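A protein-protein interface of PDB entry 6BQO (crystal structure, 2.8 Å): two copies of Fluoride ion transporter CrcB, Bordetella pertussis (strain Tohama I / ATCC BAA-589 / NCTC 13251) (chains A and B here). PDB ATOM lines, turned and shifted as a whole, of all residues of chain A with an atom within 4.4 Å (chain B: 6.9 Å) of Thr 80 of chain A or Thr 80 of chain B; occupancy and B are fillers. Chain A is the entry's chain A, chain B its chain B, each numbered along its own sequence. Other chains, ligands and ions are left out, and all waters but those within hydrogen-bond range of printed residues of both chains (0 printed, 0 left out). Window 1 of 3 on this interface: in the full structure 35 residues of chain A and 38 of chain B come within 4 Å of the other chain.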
ATOM      1  N   ALA A  42     -29.090   7.774 -14.244  1.00  0.00           N
ATOM      2  CA  ALA A  42     -30.065   8.517 -13.454  1.00  0.00           C
ATOM      3  C   ALA A  42     -29.455   9.768 -12.837  1.00  0.00           C
ATOM      4  O   ALA A  42     -30.162  10.757 -12.616  1.00  0.00           O
ATOM      5  CB  ALA A  42     -30.654   7.619 -12.367  1.00  0.00           C
ATOM      6  N   ASN A  43     -28.149   9.746 -12.557  1.00  0.00           N
ATOM      7  CA  ASN A  43     -27.496  10.898 -11.942  1.00  0.00           C
ATOM      8  C   ASN A  43     -27.182  11.978 -12.972  1.00  0.00           C
ATOM      9  O   ASN A  43     -27.453  13.162 -12.742  1.00  0.00           O
ATOM     10  CB  ASN A  43     -26.222  10.459 -11.216  1.00  0.00           C
ATOM     11  CG  ASN A  43     -26.510   9.745  -9.908  1.00  0.00           C
ATOM     12  OD1 ASN A  43     -27.560   9.940  -9.295  1.00  0.00           O
ATOM     13  ND2 ASN A  43     -25.570   8.916  -9.469  1.00  0.00           N
ATOM     14  N   GLY A  46     -30.598  13.231 -14.258  1.00  0.00           N
ATOM     15  CA  GLY A  46     -31.119  14.044 -13.174  1.00  0.00           C
ATOM     16  C   GLY A  46     -30.307  15.301 -12.940  1.00  0.00           C
ATOM     17  O   GLY A  46     -30.854  16.332 -12.536  1.00  0.00           O
ATOM     18  N   LEU A  76     -36.849  14.412  -9.310  1.00  0.00           N
ATOM     19  CA  LEU A  76     -35.389  14.399  -9.314  1.00  0.00           C
ATOM     20  C   LEU A  76     -34.822  13.981  -7.964  1.00  0.00           C
ATOM     21  O   LEU A  76     -33.734  13.395  -7.903  1.00  0.00           O
ATOM     22  CB  LEU A  76     -34.854  15.770  -9.719  1.00  0.00           C
ATOM     23  CG  LEU A  76     -35.219  16.204 -11.139  1.00  0.00           C
ATOM     24  CD1 LEU A  76     -34.525  17.507 -11.500  1.00  0.00           C
ATOM     25  CD2 LEU A  76     -34.867  15.107 -12.132  1.00  0.00           C
ATOM     26  N   GLY A  77     -35.533  14.270  -6.874  1.00  0.00           N
ATOM     27  CA  GLY A  77     -35.064  13.845  -5.567  1.00  0.00           C
ATOM     28  C   GLY A  77     -35.000  12.338  -5.425  1.00  0.00           C
ATOM     29  O   GLY A  77     -34.118  11.811  -4.740  1.00  0.00           O
ATOM     30  N   GLY A  78     -35.926  11.625  -6.064  1.00  0.00           N
ATOM     31  CA  GLY A  78     -35.941  10.177  -6.022  1.00  0.00           C
ATOM     32  C   GLY A  78     -35.229   9.552  -7.202  1.00  0.00           C
ATOM     33  O   GLY A  78     -34.766   8.410  -7.125  1.00  0.00           O
ATOM     34  N   LEU A  79     -35.131  10.293  -8.306  1.00  0.00           N
ATOM     35  CA  LEU A  79     -34.432   9.775  -9.477  1.00  0.00           C
ATOM     36  C   LEU A  79     -32.946   9.583  -9.190  1.00  0.00           C
ATOM     37  O   LEU A  79     -32.393   8.505  -9.427  1.00  0.00           O
ATOM     38  CB  LEU A  79     -34.635  10.708 -10.670  1.00  0.00           C
ATOM     39  CG  LEU A  79     -33.874  10.293 -11.930  1.00  0.00           C
ATOM     40  CD1 LEU A  79     -34.301   8.902 -12.372  1.00  0.00           C
ATOM     41  CD2 LEU A  79     -34.079  11.303 -13.046  1.00  0.00           C
ATOM     42  N   THR A  80     -32.284  10.619  -8.684  1.00  0.00           N
ATOM     43  CA  THR A  80     -30.866  10.542  -8.371  1.00  0.00           C
ATOM     44  C   THR A  80     -30.668  10.110  -6.923  1.00  0.00           C
ATOM     45  O   THR A  80     -31.524  10.338  -6.065  1.00  0.00           O
ATOM     46  CB  THR A  80     -30.179  11.889  -8.612  1.00  0.00           C
ATOM     47  OG1 THR A  80     -30.766  12.889  -7.771  1.00  0.00           O
ATOM     48  CG2 THR A  80     -30.331  12.311 -10.064  1.00  0.00           C
ATOM     49  N   THR A  81     -29.529   9.474  -6.660  1.00  0.00           N
ATOM     50  CA  THR A  81     -29.191   9.022  -5.319  1.00  0.00           C
ATOM     51  C   THR A  81     -27.714   9.253  -5.048  1.00  0.00           C
ATOM     52  O   THR A  81     -26.882   9.211  -5.959  1.00  0.00           O
ATOM     53  CB  THR A  81     -29.508   7.532  -5.102  1.00  0.00           C
ATOM     54  OG1 THR A  81     -28.900   6.752  -6.140  1.00  0.00           O
ATOM     55  CG2 THR A  81     -31.008   7.294  -5.091  1.00  0.00           C
ATOM     56  N   PHE A  82     -27.402   9.501  -3.779  1.00  0.00           N
ATOM     57  CA  PHE A  82     -26.031   9.489  -3.288  1.00  0.00           C
ATOM     58  C   PHE A  82     -25.704   8.209  -2.533  1.00  0.00           C
ATOM     59  O   PHE A  82     -24.575   7.714  -2.614  1.00  0.00           O
ATOM     60  CB  PHE A  82     -25.779  10.698  -2.380  1.00  0.00           C
ATOM     61  CG  PHE A  82     -24.513  11.442  -2.699  1.00  0.00           C
ATOM     62  CD1 PHE A  82     -23.282  10.941  -2.312  1.00  0.00           C
ATOM     63  CD2 PHE A  82     -24.556  12.642  -3.387  1.00  0.00           C
ATOM     64  CE1 PHE A  82     -22.116  11.624  -2.609  1.00  0.00           C
ATOM     65  CE2 PHE A  82     -23.395  13.330  -3.686  1.00  0.00           C
ATOM     66  CZ  PHE A  82     -22.174  12.820  -3.297  1.00  0.00           C
ATOM     67  N   SER A  83     -26.682   7.653  -1.814  1.00  0.00           N
ATOM     68  CA  SER A  83     -26.450   6.435  -1.044  1.00  0.00           C
ATOM     69  C   SER A  83     -26.046   5.276  -1.950  1.00  0.00           C
ATOM     70  O   SER A  83     -25.088   4.551  -1.659  1.00  0.00           O
ATOM     71  CB  SER A  83     -27.703   6.082  -0.243  1.00  0.00           C
ATOM     72  OG  SER A  83     -28.824   5.927  -1.097  1.00  0.00           O
ATOM     73  N   GLY B  19     -38.789   8.826   2.349  1.00  0.00           N
ATOM     74  CA  GLY B  19     -37.429   9.316   2.206  1.00  0.00           C
ATOM     75  C   GLY B  19     -37.371  10.757   1.738  1.00  0.00           C
ATOM     76  O   GLY B  19     -36.521  11.531   2.186  1.00  0.00           O
ATOM     77  N   ARG B  23     -36.047  14.151   3.602  1.00  0.00           N
ATOM     78  CA  ARG B  23     -35.099  15.014   2.906  1.00  0.00           C
ATOM     79  C   ARG B  23     -35.649  16.422   2.737  1.00  0.00           C
ATOM     80  O   ARG B  23     -34.886  17.394   2.770  1.00  0.00           O
ATOM     81  CB  ARG B  23     -34.749  14.420   1.543  1.00  0.00           C
ATOM     82  CG  ARG B  23     -33.564  15.084   0.873  1.00  0.00           C
ATOM     83  CD  ARG B  23     -33.292  14.502  -0.503  1.00  0.00           C
ATOM     84  NE  ARG B  23     -34.131  15.105  -1.532  1.00  0.00           N
ATOM     85  CZ  ARG B  23     -35.231  14.546  -2.024  1.00  0.00           C
ATOM     86  NH1 ARG B  23     -35.630  13.361  -1.585  1.00  0.00           N
ATOM     87  NH2 ARG B  23     -35.929  15.171  -2.962  1.00  0.00           N
ATOM     88  N   THR B  39     -29.063  19.361   2.854  1.00  0.00           N
ATOM     89  CA  THR B  39     -28.657  18.432   1.805  1.00  0.00           C
ATOM     90  C   THR B  39     -27.480  17.569   2.238  1.00  0.00           C
ATOM     91  O   THR B  39     -27.369  16.413   1.813  1.00  0.00           O
ATOM     92  CB  THR B  39     -28.298  19.195   0.532  1.00  0.00           C
ATOM     93  OG1 THR B  39     -29.461  19.858   0.023  1.00  0.00           O
ATOM     94  CG2 THR B  39     -27.756  18.240  -0.523  1.00  0.00           C
ATOM     95  N   ALA B  42     -28.857  14.800   4.779  1.00  0.00           N
ATOM     96  CA  ALA B  42     -29.596  13.744   4.097  1.00  0.00           C
ATOM     97  C   ALA B  42     -28.650  12.756   3.425  1.00  0.00           C
ATOM     98  O   ALA B  42     -28.851  11.539   3.508  1.00  0.00           O
ATOM     99  CB  ALA B  42     -30.560  14.350   3.076  1.00  0.00           C
ATOM    100  N   ASN B  43     -27.607  13.260   2.761  1.00  0.00           N
ATOM    101  CA  ASN B  43     -26.678  12.370   2.075  1.00  0.00           C
ATOM    102  C   ASN B  43     -25.764  11.649   3.061  1.00  0.00           C
ATOM    103  O   ASN B  43     -25.566  10.434   2.951  1.00  0.00           O
ATOM    104  CB  ASN B  43     -25.866  13.157   1.046  1.00  0.00           C
ATOM    105  CG  ASN B  43     -26.713  13.634  -0.120  1.00  0.00           C
ATOM    106  OD1 ASN B  43     -27.940  13.563  -0.077  1.00  0.00           O
ATOM    107  ND2 ASN B  43     -26.061  14.124  -1.168  1.00  0.00           N
ATOM    108  N   LEU B  44     -25.206  12.371   4.034  1.00  0.00           N
ATOM    109  CA  LEU B  44     -24.321  11.733   5.004  1.00  0.00           C
ATOM    110  C   LEU B  44     -25.067  10.692   5.828  1.00  0.00           C
ATOM    111  O   LEU B  44     -24.583   9.569   6.015  1.00  0.00           O
ATOM    112  CB  LEU B  44     -23.685  12.784   5.913  1.00  0.00           C
ATOM    113  CG  LEU B  44     -22.294  13.263   5.497  1.00  0.00           C
ATOM    114  CD1 LEU B  44     -22.345  13.936   4.137  1.00  0.00           C
ATOM    115  CD2 LEU B  44     -21.718  14.198   6.547  1.00  0.00           C
ATOM    116  N   VAL B  45     -26.245  11.048   6.340  1.00  0.00           N
ATOM    117  CA  VAL B  45     -27.043  10.083   7.092  1.00  0.00           C
ATOM    118  C   VAL B  45     -27.412   8.906   6.203  1.00  0.00           C
ATOM    119  O   VAL B  45     -27.297   7.741   6.602  1.00  0.00           O
ATOM    120  CB  VAL B  45     -28.296  10.757   7.680  1.00  0.00           C
ATOM    121  CG1 VAL B  45     -29.166   9.725   8.378  1.00  0.00           C
ATOM    122  CG2 VAL B  45     -27.903  11.868   8.642  1.00  0.00           C
ATOM    123  N   GLY B  46     -27.862   9.194   4.980  1.00  0.00           N
ATOM    124  CA  GLY B  46     -28.205   8.124   4.059  1.00  0.00           C
ATOM    125  C   GLY B  46     -27.010   7.268   3.690  1.00  0.00           C
ATOM    126  O   GLY B  46     -27.103   6.039   3.648  1.00  0.00           O
ATOM    127  N   GLY B  47     -25.871   7.906   3.416  1.00  0.00           N
ATOM    128  CA  GLY B  47     -24.670   7.149   3.104  1.00  0.00           C
ATOM    129  C   GLY B  47     -24.279   6.197   4.217  1.00  0.00           C
ATOM    130  O   GLY B  47     -23.830   5.076   3.961  1.00  0.00           O
ATOM    131  N   ILE B  50     -27.100   3.206   4.291  1.00  0.00           N
ATOM    132  CA  ILE B  50     -26.979   2.206   3.233  1.00  0.00           C
ATOM    133  C   ILE B  50     -25.829   1.256   3.542  1.00  0.00           C
ATOM    134  O   ILE B  50     -25.912   0.050   3.278  1.00  0.00           O
ATOM    135  CB  ILE B  50     -26.815   2.879   1.857  1.00  0.00           C
ATOM    136  CG1 ILE B  50     -27.003   1.846   0.743  1.00  0.00           C
ATOM    137  CG2 ILE B  50     -25.456   3.547   1.740  1.00  0.00           C
ATOM    138  CD1 ILE B  50     -26.983   2.434  -0.647  1.00  0.00           C
ATOM    139  N   PHE B  75     -36.470   4.073   0.666  1.00  0.00           N
ATOM    140  CA  PHE B  75     -36.153   5.092   1.659  1.00  0.00           C
ATOM    141  C   PHE B  75     -34.846   5.805   1.337  1.00  0.00           C
ATOM    142  O   PHE B  75     -34.847   7.000   1.023  1.00  0.00           O
ATOM    143  CB  PHE B  75     -36.091   4.461   3.053  1.00  0.00           C
ATOM    144  CG  PHE B  75     -36.052   5.461   4.171  1.00  0.00           C
ATOM    145  CD1 PHE B  75     -37.027   6.438   4.276  1.00  0.00           C
ATOM    146  CD2 PHE B  75     -35.050   5.414   5.128  1.00  0.00           C
ATOM    147  CE1 PHE B  75     -36.996   7.358   5.309  1.00  0.00           C
ATOM    148  CE2 PHE B  75     -35.016   6.329   6.164  1.00  0.00           C
ATOM    149  CZ  PHE B  75     -35.990   7.302   6.255  1.00  0.00           C
ATOM    150  N   LEU B  76     -33.724   5.085   1.410  1.00  0.00           N
ATOM    151  CA  LEU B  76     -32.431   5.708   1.147  1.00  0.00           C
ATOM    152  C   LEU B  76     -32.336   6.266  -0.266  1.00  0.00           C
ATOM    153  O   LEU B  76     -31.485   7.124  -0.525  1.00  0.00           O
ATOM    154  CB  LEU B  76     -31.304   4.706   1.391  1.00  0.00           C
ATOM    155  CG  LEU B  76     -31.178   4.226   2.836  1.00  0.00           C
ATOM    156  CD1 LEU B  76     -30.049   3.222   2.976  1.00  0.00           C
ATOM    157  CD2 LEU B  76     -30.969   5.405   3.771  1.00  0.00           C
ATOM    158  N   GLY B  77     -33.184   5.800  -1.187  1.00  0.00           N
ATOM    159  CA  GLY B  77     -33.207   6.363  -2.524  1.00  0.00           C
ATOM    160  C   GLY B  77     -33.926   7.689  -2.629  1.00  0.00           C
ATOM    161  O   GLY B  77     -33.698   8.431  -3.588  1.00  0.00           O
ATOM    162  N   GLY B  78     -34.797   7.998  -1.672  1.00  0.00           N
ATOM    163  CA  GLY B  78     -35.466   9.281  -1.641  1.00  0.00           C
ATOM    164  C   GLY B  78     -34.830  10.215  -0.634  1.00  0.00           C
ATOM    165  O   GLY B  78     -35.009  11.435  -0.702  1.00  0.00           O
ATOM    166  N   LEU B  79     -34.079   9.645   0.309  1.00  0.00           N
ATOM    167  CA  LEU B  79     -33.389  10.455   1.307  1.00  0.00           C
ATOM    168  C   LEU B  79     -32.171  11.144   0.703  1.00  0.00           C
ATOM    169  O   LEU B  79     -32.037  12.372   0.770  1.00  0.00           O
ATOM    170  CB  LEU B  79     -32.985   9.587   2.498  1.00  0.00           C
ATOM    171  CG  LEU B  79     -32.275  10.320   3.637  1.00  0.00           C
ATOM    172  CD1 LEU B  79     -33.179  11.389   4.228  1.00  0.00           C
ATOM    173  CD2 LEU B  79     -31.831   9.340   4.708  1.00  0.00           C
ATOM    174  N   THR B  80     -31.262  10.370   0.116  1.00  0.00           N
ATOM    175  CA  THR B  80     -30.094  10.962  -0.513  1.00  0.00           C
ATOM    176  C   THR B  80     -30.492  11.629  -1.827  1.00  0.00           C
ATOM    177  O   THR B  80     -31.615  11.484  -2.317  1.00  0.00           O
ATOM    178  CB  THR B  80     -29.013   9.906  -0.747  1.00  0.00           C
ATOM    179  OG1 THR B  80     -29.426   9.014  -1.790  1.00  0.00           O
ATOM    180  CG2 THR B  80     -28.777   9.106   0.526  1.00  0.00           C
ATOM    181  N   THR B  81     -29.555  12.385  -2.399  1.00  0.00           N
ATOM    182  CA  THR B  81     -29.831  13.085  -3.647  1.00  0.00           C
ATOM    183  C   THR B  81     -28.553  13.602  -4.292  1.00  0.00           C
ATOM    184  O   THR B  81     -27.723  14.233  -3.631  1.00  0.00           O
ATOM    185  CB  THR B  81     -30.804  14.246  -3.416  1.00  0.00           C
ATOM    186  OG1 THR B  81     -31.056  14.917  -4.658  1.00  0.00           O
ATOM    187  CG2 THR B  81     -30.227  15.245  -2.418  1.00  0.00           C
ATOM    188  N   PHE B  82     -28.387  13.327  -5.585  1.00  0.00           N
ATOM    189  CA  PHE B  82     -27.289  13.885  -6.362  1.00  0.00           C
ATOM    190  C   PHE B  82     -27.698  15.149  -7.100  1.00  0.00           C
ATOM    191  O   PHE B  82     -26.868  16.047  -7.289  1.00  0.00           O
ATOM    192  CB  PHE B  82     -26.779  12.850  -7.370  1.00  0.00           C
ATOM    193  CG  PHE B  82     -25.285  12.711  -7.401  1.00  0.00           C
ATOM    194  CD1 PHE B  82     -24.520  13.471  -8.272  1.00  0.00           C
ATOM    195  CD2 PHE B  82     -24.643  11.811  -6.567  1.00  0.00           C
ATOM    196  CE1 PHE B  82     -23.144  13.340  -8.304  1.00  0.00           C
ATOM    197  CE2 PHE B  82     -23.268  11.675  -6.593  1.00  0.00           C
ATOM    198  CZ  PHE B  82     -22.517  12.440  -7.463  1.00  0.00           C
ATOM    199  N   SER B  83     -28.965  15.240  -7.511  1.00  0.00           N
ATOM    200  CA  SER B  83     -29.425  16.384  -8.289  1.00  0.00           C
ATOM    201  C   SER B  83     -29.263  17.684  -7.509  1.00  0.00           C
ATOM    202  O   SER B  83     -28.517  18.581  -7.918  1.00  0.00           O
ATOM    203  CB  SER B  83     -30.882  16.174  -8.709  1.00  0.00           C
ATOM    204  OG  SER B  83     -31.712  15.942  -7.585  1.00  0.00           O
ATOM    205  N   THR B  84     -29.958  17.805  -6.374  1.00  0.00           N
ATOM    206  CA  THR B  84     -29.904  19.050  -5.614  1.00  0.00           C
ATOM    207  C   THR B  84     -28.473  19.394  -5.220  1.00  0.00           C
ATOM    208  O   THR B  84     -28.084  20.568  -5.230  1.00  0.00           O
ATOM    209  CB  THR B  84     -30.799  18.958  -4.377  1.00  0.00           C
ATOM    210  OG1 THR B  84     -30.197  18.092  -3.407  1.00  0.00           O
ATOM    211  CG2 THR B  84     -32.170  18.413  -4.752  1.00  0.00           C
ATOM    212  N   SER B 112     -19.721  10.862   2.289  1.00  0.00           N
ATOM    213  CA  SER B 112     -20.622   9.741   2.043  1.00  0.00           C
ATOM    214  C   SER B 112     -19.865   8.419   2.056  1.00  0.00           C
ATOM    215  O   SER B 112     -20.265   7.466   2.737  1.00  0.00           O
ATOM    216  CB  SER B 112     -21.346   9.939   0.712  1.00  0.00           C
ATOM    217  OG  SER B 112     -22.372   8.977   0.544  1.00  0.00           O
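Leu 76 of chain A touches Ser 83 of chain B, and with the chains exchanged Ser 83 of chain A touches Leu 76 of chain B. Gly 77 of chain A touches Thr 80 of chain B, and with the chains exchanged Thr 80 of chain A touches Gly 77 of chain B. Gly 78 of chain A touches Gly 77 of chain B, but with the chains exchanged Gly 77 of chain A does not touch Gly 78 of chain B (4.2 Å). Thr 81 of chain A touches Phe 82 of chain B, and with the chains exchanged Phe 82 of chain A touches Thr 81 of chain B. Of the 24 pairs that touch across the chains among the printed residues, 19 have their exchanged pair printed and touching as well.
The side-chain amide oxygen (OD1) of Asn 43 of chain A lies within hydrogen-bond range of the backbone NH (N) of Thr 81 of chain A (3.3 Å). The backbone carbonyl oxygen (O) of Thr 81 of chain B sits at hydrogen-bond distance from the side-chain amide nitrogen (ND2) of Asn 43 of chain B. OG1 of Thr 80 of chain B lies within hydrogen-bond range of O of Leu 76 of chain B, at 3.1 Å. The backbone carbonyl oxygen of Leu 76 of chain A is in hydrogen-bond range of the side-chain hydroxyl of Thr 80 of chain A (3.0 Å). The side-chain amide oxygen of Asn 43 of chain B sits close to the backbone carbonyl oxygen of Thr 39 of chain B. OG1 of Thr 81 of chain B lies within hydrogen-bond range of OG of Ser 83 of chain B, at 3.2 Å.
The side-chain hydroxyl of Thr 80 of chain A lies within hydrogen-bond range of the backbone NH of Phe 82 of chain B. The side-chain hydroxyl of Thr 80 of chain A lies within hydrogen-bond range of the backbone NH of Ser 83 of chain B (3.0 Å). O of Leu 76 of chain B sits at hydrogen-bond distance from OG of Ser 83 of chain A (3.0 Å). The backbone carbonyl oxygen (O) of Leu 76 of chain A sits at hydrogen-bond distance from the side-chain hydroxyl (OG) of Ser 83 of chain B, 3.3 Å away. The side-chain hydroxyl of Thr 80 of chain B lies within hydrogen-bond range of the backbone NH of Ser 83 of chain A (3.1 Å). O of Thr 80 of chain B lies close to O of Gly 77 of chain A, 3.5 Å away. The side-chain hydroxyl of Thr 80 of chain B is in hydrogen-bond range of the backbone NH of Phe 82 of chain A (2.9 Å).
Thr 80 of chain A touches just these residues of chain B: Gly 77, Thr 80, Thr 81, Phe 82 and Ser 83. Gly 19 of chain B touches none of the printed residues of chain A. Of the printed residues of chain A, Gly 46 of chain B touches Ser 83. Thr 80 of chain B touches just these residues of chain A: Gly 77, Thr 80, Thr 81, Phe 82 and Ser 83. Of the printed residues of chain A, Thr 81 of chain B touches Thr 80 and Phe 82. The nearest printed residue of chain A that does not touch Gly 77 of chain B is Ser 83 of chain A (4.4 Å).
CB of Ser 83 of chain B touches O of Gly 46 of chain A, at 3.8 Å. Gly 77 of chain A touches Arg 23 of chain B. O of Thr 80 of chain A touches O of Gly 77 of chain B, 3.8 Å away. Thr 80 of chain A touches Thr 80 of chain B. CA of Thr 81 of chain A touches OG1 of Thr 80 of chain B, 3.5 Å away. Phe 82 of chain A touches Asn 43 of chain B (CD2 to ND2, 3.1 Å). Phe 82 of chain A touches Thr 81 of chain B. CD2 of Phe 82 of chain A touches CD2 of Phe 82 of chain B (3.3 Å). Ser 112 of chain B touches Phe 82 of chain A. Ser 83 of chain A touches Gly 46 of chain B (CB to O, 3.9 Å).
Of the 11 printed residues of chain A, 9 touch a printed residue of chain B. Hydrophobic or aromatic side chains of chain A that line the printed part of chain B: Leu 76 and Phe 82. Hydrophobic or aromatic side chains of chain B that line the printed part of chain A: Ile 50, Leu 76 and Phe 82. Among the printed residues, 24 pairs touch across the chains. Among the printed residues, no Asp or Glu carboxylate lies within 4 Å of a Lys or Arg side-chain nitrogen of the other chain.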
